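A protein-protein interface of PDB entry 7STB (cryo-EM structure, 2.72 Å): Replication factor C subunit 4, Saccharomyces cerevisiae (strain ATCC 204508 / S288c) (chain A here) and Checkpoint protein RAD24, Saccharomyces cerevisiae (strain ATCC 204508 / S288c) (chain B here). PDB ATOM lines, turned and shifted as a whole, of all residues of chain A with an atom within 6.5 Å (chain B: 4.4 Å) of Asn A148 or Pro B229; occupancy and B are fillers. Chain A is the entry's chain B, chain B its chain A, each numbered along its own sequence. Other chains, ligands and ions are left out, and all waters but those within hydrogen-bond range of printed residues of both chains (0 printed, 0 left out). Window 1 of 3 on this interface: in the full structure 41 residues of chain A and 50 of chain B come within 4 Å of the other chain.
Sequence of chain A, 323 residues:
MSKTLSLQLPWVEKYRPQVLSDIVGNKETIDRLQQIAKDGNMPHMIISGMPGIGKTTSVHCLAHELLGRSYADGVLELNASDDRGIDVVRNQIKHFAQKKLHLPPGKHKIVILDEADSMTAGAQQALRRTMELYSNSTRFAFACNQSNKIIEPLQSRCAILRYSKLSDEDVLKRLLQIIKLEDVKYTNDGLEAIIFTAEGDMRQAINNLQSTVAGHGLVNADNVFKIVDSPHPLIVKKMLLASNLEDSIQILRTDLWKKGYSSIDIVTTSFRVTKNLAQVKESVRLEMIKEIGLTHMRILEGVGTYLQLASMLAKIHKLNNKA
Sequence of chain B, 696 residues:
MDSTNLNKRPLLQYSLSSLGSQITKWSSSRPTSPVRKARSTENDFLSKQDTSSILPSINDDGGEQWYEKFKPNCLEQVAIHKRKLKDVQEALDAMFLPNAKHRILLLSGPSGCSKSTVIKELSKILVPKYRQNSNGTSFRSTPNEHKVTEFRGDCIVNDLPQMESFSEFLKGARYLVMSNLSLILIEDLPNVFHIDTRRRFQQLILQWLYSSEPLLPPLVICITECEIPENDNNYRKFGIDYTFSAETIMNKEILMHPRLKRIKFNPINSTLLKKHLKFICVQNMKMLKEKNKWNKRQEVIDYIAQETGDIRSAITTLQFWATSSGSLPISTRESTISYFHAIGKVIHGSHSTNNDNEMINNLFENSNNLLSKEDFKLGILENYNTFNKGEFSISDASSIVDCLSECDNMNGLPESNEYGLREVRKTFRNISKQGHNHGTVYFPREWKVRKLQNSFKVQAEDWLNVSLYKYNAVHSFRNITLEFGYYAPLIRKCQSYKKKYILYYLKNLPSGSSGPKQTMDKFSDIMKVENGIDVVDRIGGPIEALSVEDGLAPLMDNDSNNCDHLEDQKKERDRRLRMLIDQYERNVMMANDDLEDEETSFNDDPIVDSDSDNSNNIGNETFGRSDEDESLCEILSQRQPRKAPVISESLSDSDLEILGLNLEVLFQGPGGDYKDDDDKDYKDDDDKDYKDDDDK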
ATOM      1  N   ASP A 117      11.861  -2.413  12.735  1.00  0.00           N
ATOM      2  CA  ASP A 117      11.597  -1.458  13.803  1.00  0.00           C
ATOM      3  C   ASP A 117      11.746  -0.007  13.356  1.00  0.00           C
ATOM      4  O   ASP A 117      11.729   0.889  14.208  1.00  0.00           O
ATOM      5  CB  ASP A 117      12.522  -1.737  14.992  1.00  0.00           C
ATOM      6  CG  ASP A 117      13.988  -1.561  14.649  1.00  0.00           C
ATOM      7  OD1 ASP A 117      14.300  -1.261  13.477  1.00  0.00           O
ATOM      8  OD2 ASP A 117      14.832  -1.724  15.556  1.00  0.00           O
ATOM      9  N   GLN A 124       2.721  -0.126   8.871  1.00  0.00           N
ATOM     10  CA  GLN A 124       2.364  -1.241   9.744  1.00  0.00           C
ATOM     11  C   GLN A 124       0.852  -1.443   9.799  1.00  0.00           C
ATOM     12  O   GLN A 124       0.371  -2.582   9.850  1.00  0.00           O
ATOM     13  CB  GLN A 124       2.928  -1.004  11.144  1.00  0.00           C
ATOM     14  CG  GLN A 124       4.446  -0.928  11.185  1.00  0.00           C
ATOM     15  CD  GLN A 124       5.006  -1.164  12.571  1.00  0.00           C
ATOM     16  OE1 GLN A 124       4.701  -2.168  13.213  1.00  0.00           O
ATOM     17  NE2 GLN A 124       5.835  -0.238  13.040  1.00  0.00           N
ATOM     18  N   CYS A 144      14.292  -7.318  14.037  1.00  0.00           N
ATOM     19  CA  CYS A 144      14.457  -6.028  14.689  1.00  0.00           C
ATOM     20  C   CYS A 144      15.382  -6.193  15.885  1.00  0.00           C
ATOM     21  O   CYS A 144      15.863  -7.290  16.180  1.00  0.00           O
ATOM     22  CB  CYS A 144      13.102  -5.450  15.109  1.00  0.00           C
ATOM     23  SG  CYS A 144      12.018  -6.632  15.947  1.00  0.00           S
ATOM     24  N   GLN A 146      14.418  -4.225  18.960  1.00  0.00           N
ATOM     25  CA  GLN A 146      13.423  -4.128  20.020  1.00  0.00           C
ATOM     26  C   GLN A 146      12.104  -4.666  19.489  1.00  0.00           C
ATOM     27  O   GLN A 146      11.605  -4.189  18.463  1.00  0.00           O
ATOM     28  CB  GLN A 146      13.269  -2.683  20.497  1.00  0.00           C
ATOM     29  CG  GLN A 146      14.344  -2.232  21.472  1.00  0.00           C
ATOM     30  CD  GLN A 146      14.308  -2.996  22.781  1.00  0.00           C
ATOM     31  OE1 GLN A 146      15.318  -3.545  23.220  1.00  0.00           O
ATOM     32  NE2 GLN A 146      13.140  -3.034  23.413  1.00  0.00           N
ATOM     33  N   SER A 147      11.540  -5.654  20.186  1.00  0.00           N
ATOM     34  CA  SER A 147      10.290  -6.257  19.733  1.00  0.00           C
ATOM     35  C   SER A 147       9.112  -5.306  19.902  1.00  0.00           C
ATOM     36  O   SER A 147       8.158  -5.359  19.117  1.00  0.00           O
ATOM     37  CB  SER A 147      10.032  -7.558  20.491  1.00  0.00           C
ATOM     38  OG  SER A 147       8.967  -8.285  19.904  1.00  0.00           O
ATOM     39  N   ASN A 148       9.155  -4.436  20.914  1.00  0.00           N
ATOM     40  CA  ASN A 148       8.046  -3.522  21.158  1.00  0.00           C
ATOM     41  C   ASN A 148       7.877  -2.502  20.041  1.00  0.00           C
ATOM     42  O   ASN A 148       6.823  -1.863  19.959  1.00  0.00           O
ATOM     43  CB  ASN A 148       8.245  -2.800  22.490  1.00  0.00           C
ATOM     44  CG  ASN A 148       9.507  -1.964  22.518  1.00  0.00           C
ATOM     45  OD1 ASN A 148      10.615  -2.494  22.607  1.00  0.00           O
ATOM     46  ND2 ASN A 148       9.347  -0.648  22.441  1.00  0.00           N
ATOM     47  N   LYS A 149       8.884  -2.333  19.181  1.00  0.00           N
ATOM     48  CA  LYS A 149       8.784  -1.380  18.084  1.00  0.00           C
ATOM     49  C   LYS A 149       7.781  -1.809  17.022  1.00  0.00           C
ATOM     50  O   LYS A 149       7.449  -1.000  16.150  1.00  0.00           O
ATOM     51  CB  LYS A 149      10.158  -1.176  17.445  1.00  0.00           C
ATOM     52  CG  LYS A 149      11.214  -0.609  18.392  1.00  0.00           C
ATOM     53  CD  LYS A 149      10.855   0.775  18.924  1.00  0.00           C
ATOM     54  CE  LYS A 149      10.861   1.830  17.831  1.00  0.00           C
ATOM     55  NZ  LYS A 149      12.218   2.035  17.255  1.00  0.00           N
ATOM     56  N   ILE A 150       7.305  -3.048  17.067  1.00  0.00           N
ATOM     57  CA  ILE A 150       6.256  -3.517  16.171  1.00  0.00           C
ATOM     58  C   ILE A 150       4.915  -3.328  16.866  1.00  0.00           C
ATOM     59  O   ILE A 150       4.758  -3.689  18.038  1.00  0.00           O
ATOM     60  CB  ILE A 150       6.476  -4.989  15.784  1.00  0.00           C
ATOM     61  CG1 ILE A 150       7.946  -5.246  15.429  1.00  0.00           C
ATOM     62  CG2 ILE A 150       5.573  -5.375  14.624  1.00  0.00           C
ATOM     63  CD1 ILE A 150       8.458  -4.425  14.263  1.00  0.00           C
ATOM     64  N   ILE A 151       3.948  -2.753  16.149  1.00  0.00           N
ATOM     65  CA  ILE A 151       2.662  -2.455  16.763  1.00  0.00           C
ATOM     66  C   ILE A 151       2.002  -3.745  17.246  1.00  0.00           C
ATOM     67  O   ILE A 151       2.157  -4.817  16.646  1.00  0.00           O
ATOM     68  CB  ILE A 151       1.748  -1.697  15.784  1.00  0.00           C
ATOM     69  CG1 ILE A 151       1.532  -2.502  14.501  1.00  0.00           C
ATOM     70  CG2 ILE A 151       2.343  -0.338  15.456  1.00  0.00           C
ATOM     71  CD1 ILE A 151       0.417  -1.965  13.631  1.00  0.00           C
ATOM     72  N   GLU A 152       1.259  -3.635  18.347  1.00  0.00           N
ATOM     73  CA  GLU A 152       0.656  -4.816  18.958  1.00  0.00           C
ATOM     74  C   GLU A 152      -0.213  -5.618  17.999  1.00  0.00           C
ATOM     75  O   GLU A 152      -0.171  -6.859  18.066  1.00  0.00           O
ATOM     76  CB  GLU A 152      -0.156  -4.400  20.190  1.00  0.00           C
ATOM     77  CG  GLU A 152       0.688  -3.866  21.333  1.00  0.00           C
ATOM     78  CD  GLU A 152      -0.149  -3.448  22.524  1.00  0.00           C
ATOM     79  OE1 GLU A 152      -1.392  -3.458  22.412  1.00  0.00           O
ATOM     80  OE2 GLU A 152       0.437  -3.113  23.575  1.00  0.00           O
ATOM     81  N   GLN A 155       2.167  -7.837  16.278  1.00  0.00           N
ATOM     82  CA  GLN A 155       2.763  -8.802  17.195  1.00  0.00           C
ATOM     83  C   GLN A 155       1.801  -9.936  17.515  1.00  0.00           C
ATOM     84  O   GLN A 155       2.230 -11.080  17.703  1.00  0.00           O
ATOM     85  CB  GLN A 155       3.187  -8.105  18.486  1.00  0.00           C
ATOM     86  CG  GLN A 155       4.318  -7.116  18.320  1.00  0.00           C
ATOM     87  CD  GLN A 155       4.885  -6.666  19.649  1.00  0.00           C
ATOM     88  OE1 GLN A 155       4.941  -7.438  20.605  1.00  0.00           O
ATOM     89  NE2 GLN A 155       5.305  -5.411  19.718  1.00  0.00           N
ATOM     90  N   GLU B 227      -0.286   1.744  21.170  1.00  0.00           N
ATOM     91  CA  GLU B 227       0.702   2.811  21.169  1.00  0.00           C
ATOM     92  C   GLU B 227       1.503   2.803  19.873  1.00  0.00           C
ATOM     93  O   GLU B 227       1.651   1.770  19.213  1.00  0.00           O
ATOM     94  CB  GLU B 227       1.651   2.670  22.360  1.00  0.00           C
ATOM     95  CG  GLU B 227       0.995   2.892  23.711  1.00  0.00           C
ATOM     96  CD  GLU B 227       1.968   2.724  24.861  1.00  0.00           C
ATOM     97  OE1 GLU B 227       3.121   2.314  24.611  1.00  0.00           O
ATOM     98  OE2 GLU B 227       1.583   3.006  26.015  1.00  0.00           O
ATOM     99  N   ILE B 228       2.019   3.974  19.512  1.00  0.00           N
ATOM    100  CA  ILE B 228       2.867   4.139  18.334  1.00  0.00           C
ATOM    101  C   ILE B 228       4.311   4.244  18.821  1.00  0.00           C
ATOM    102  O   ILE B 228       4.666   5.255  19.447  1.00  0.00           O
ATOM    103  CB  ILE B 228       2.465   5.374  17.519  1.00  0.00           C
ATOM    104  CG1 ILE B 228       1.000   5.280  17.081  1.00  0.00           C
ATOM    105  CG2 ILE B 228       3.375   5.532  16.310  1.00  0.00           C
ATOM    106  CD1 ILE B 228       0.660   4.026  16.299  1.00  0.00           C
ATOM    107  N   PRO B 229       5.162   3.247  18.570  1.00  0.00           N
ATOM    108  CA  PRO B 229       6.543   3.329  19.057  1.00  0.00           C
ATOM    109  C   PRO B 229       7.281   4.525  18.472  1.00  0.00           C
ATOM    110  O   PRO B 229       7.044   4.936  17.334  1.00  0.00           O
ATOM    111  CB  PRO B 229       7.164   2.006  18.593  1.00  0.00           C
ATOM    112  CG  PRO B 229       6.010   1.092  18.384  1.00  0.00           C
ATOM    113  CD  PRO B 229       4.889   1.958  17.913  1.00  0.00           C
ATOM    114  N   GLU B 230       8.185   5.085  19.275  1.00  0.00           N
ATOM    115  CA  GLU B 230       8.989   6.223  18.852  1.00  0.00           C
ATOM    116  C   GLU B 230       9.844   5.845  17.649  1.00  0.00           C
ATOM    117  O   GLU B 230      10.768   5.034  17.769  1.00  0.00           O
ATOM    118  CB  GLU B 230       9.871   6.709  20.005  1.00  0.00           C
ATOM    119  CG  GLU B 230      10.700   7.947  19.692  1.00  0.00           C
ATOM    120  CD  GLU B 230       9.852   9.191  19.511  1.00  0.00           C
ATOM    121  OE1 GLU B 230       8.752   9.253  20.101  1.00  0.00           O
ATOM    122  OE2 GLU B 230      10.286  10.106  18.782  1.00  0.00           O
ATOM    123  N   ASN B 231       9.547   6.428  16.492  1.00  0.00           N
ATOM    124  CA  ASN B 231      10.233   6.112  15.250  1.00  0.00           C
ATOM    125  C   ASN B 231      11.082   7.292  14.795  1.00  0.00           C
ATOM    126  O   ASN B 231      10.752   8.457  15.033  1.00  0.00           O
ATOM    127  CB  ASN B 231       9.230   5.739  14.152  1.00  0.00           C
ATOM    128  CG  ASN B 231       9.861   4.932  13.035  1.00  0.00           C
ATOM    129  OD1 ASN B 231      11.026   4.542  13.115  1.00  0.00           O
ATOM    130  ND2 ASN B 231       9.091   4.678  11.982  1.00  0.00           N
ATOM    131  N   ASN B 369       7.642   6.065  25.953  1.00  0.00           N
ATOM    132  CA  ASN B 369       6.772   7.101  25.404  1.00  0.00           C
ATOM    133  C   ASN B 369       5.831   7.648  26.469  1.00  0.00           C
ATOM    134  O   ASN B 369       5.662   8.866  26.600  1.00  0.00           O
ATOM    135  CB  ASN B 369       5.977   6.544  24.223  1.00  0.00           C
ATOM    136  CG  ASN B 369       6.821   6.373  22.979  1.00  0.00           C
ATOM    137  OD1 ASN B 369       7.676   7.205  22.674  1.00  0.00           O
ATOM    138  ND2 ASN B 369       6.585   5.289  22.250  1.00  0.00           N
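The backbone carbonyl oxygen (O) of Glu B230 sits close to the side-chain amino group (NZ) of Lys A149.
The side-chain amide nitrogen (ND2) of Asn B369 sits close to the backbone NH (N) of Glu B230, 3.4 Å away. NZ of Lys A149 sits at hydrogen-bond distance from O of Asp A117 (3.3 Å). NE2 of Gln A146 lies within hydrogen-bond range of OD1 of Asn A148 (2.7 Å).
OD1 of Asn B231 touches O of Asp A117, 3.9 Å away. O of Asn A148 touches CG of Pro B229, 3.4 Å away. O of Lys A149 touches CG of Pro B229 (3.4 Å).
Asn A148 touches just one residue of chain B: Pro B229 (3.4 Å). Pro B229 touches just these residues of chain A: Asn A148 (3.4 Å) and Lys A149 (3.4 Å). Of the printed residues of chain A, Glu B230 touches Lys A149 (3.2 Å). Of the printed residues of chain B, Lys A149 touches Pro B229 (3.4 Å) and Glu B230 (3.2 Å). Of the printed residues of chain A, Asn B231 touches Asp A117 (3.9 Å). Of the printed residues of chain B, Asp A117 touches Asn B231. Gln A124 touches none of the printed residues of chain B. Glu B227 touches none of the printed residues of chain A. The nearest printed residue of chain B that does not touch Asn A148 is Glu B227 (6.4 Å).
Hydrophobic or aromatic side chains of chain B within 4 Å of the printed part of chain A: Pro B229. Printed residues of chain A that touch a printed residue of chain B: Asp A117, Asn A148 and Lys A149. Among the printed residues, no Asp or Glu carboxylate lies within 4 Å of a Lys or Arg side-chain nitrogen of the other chain.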
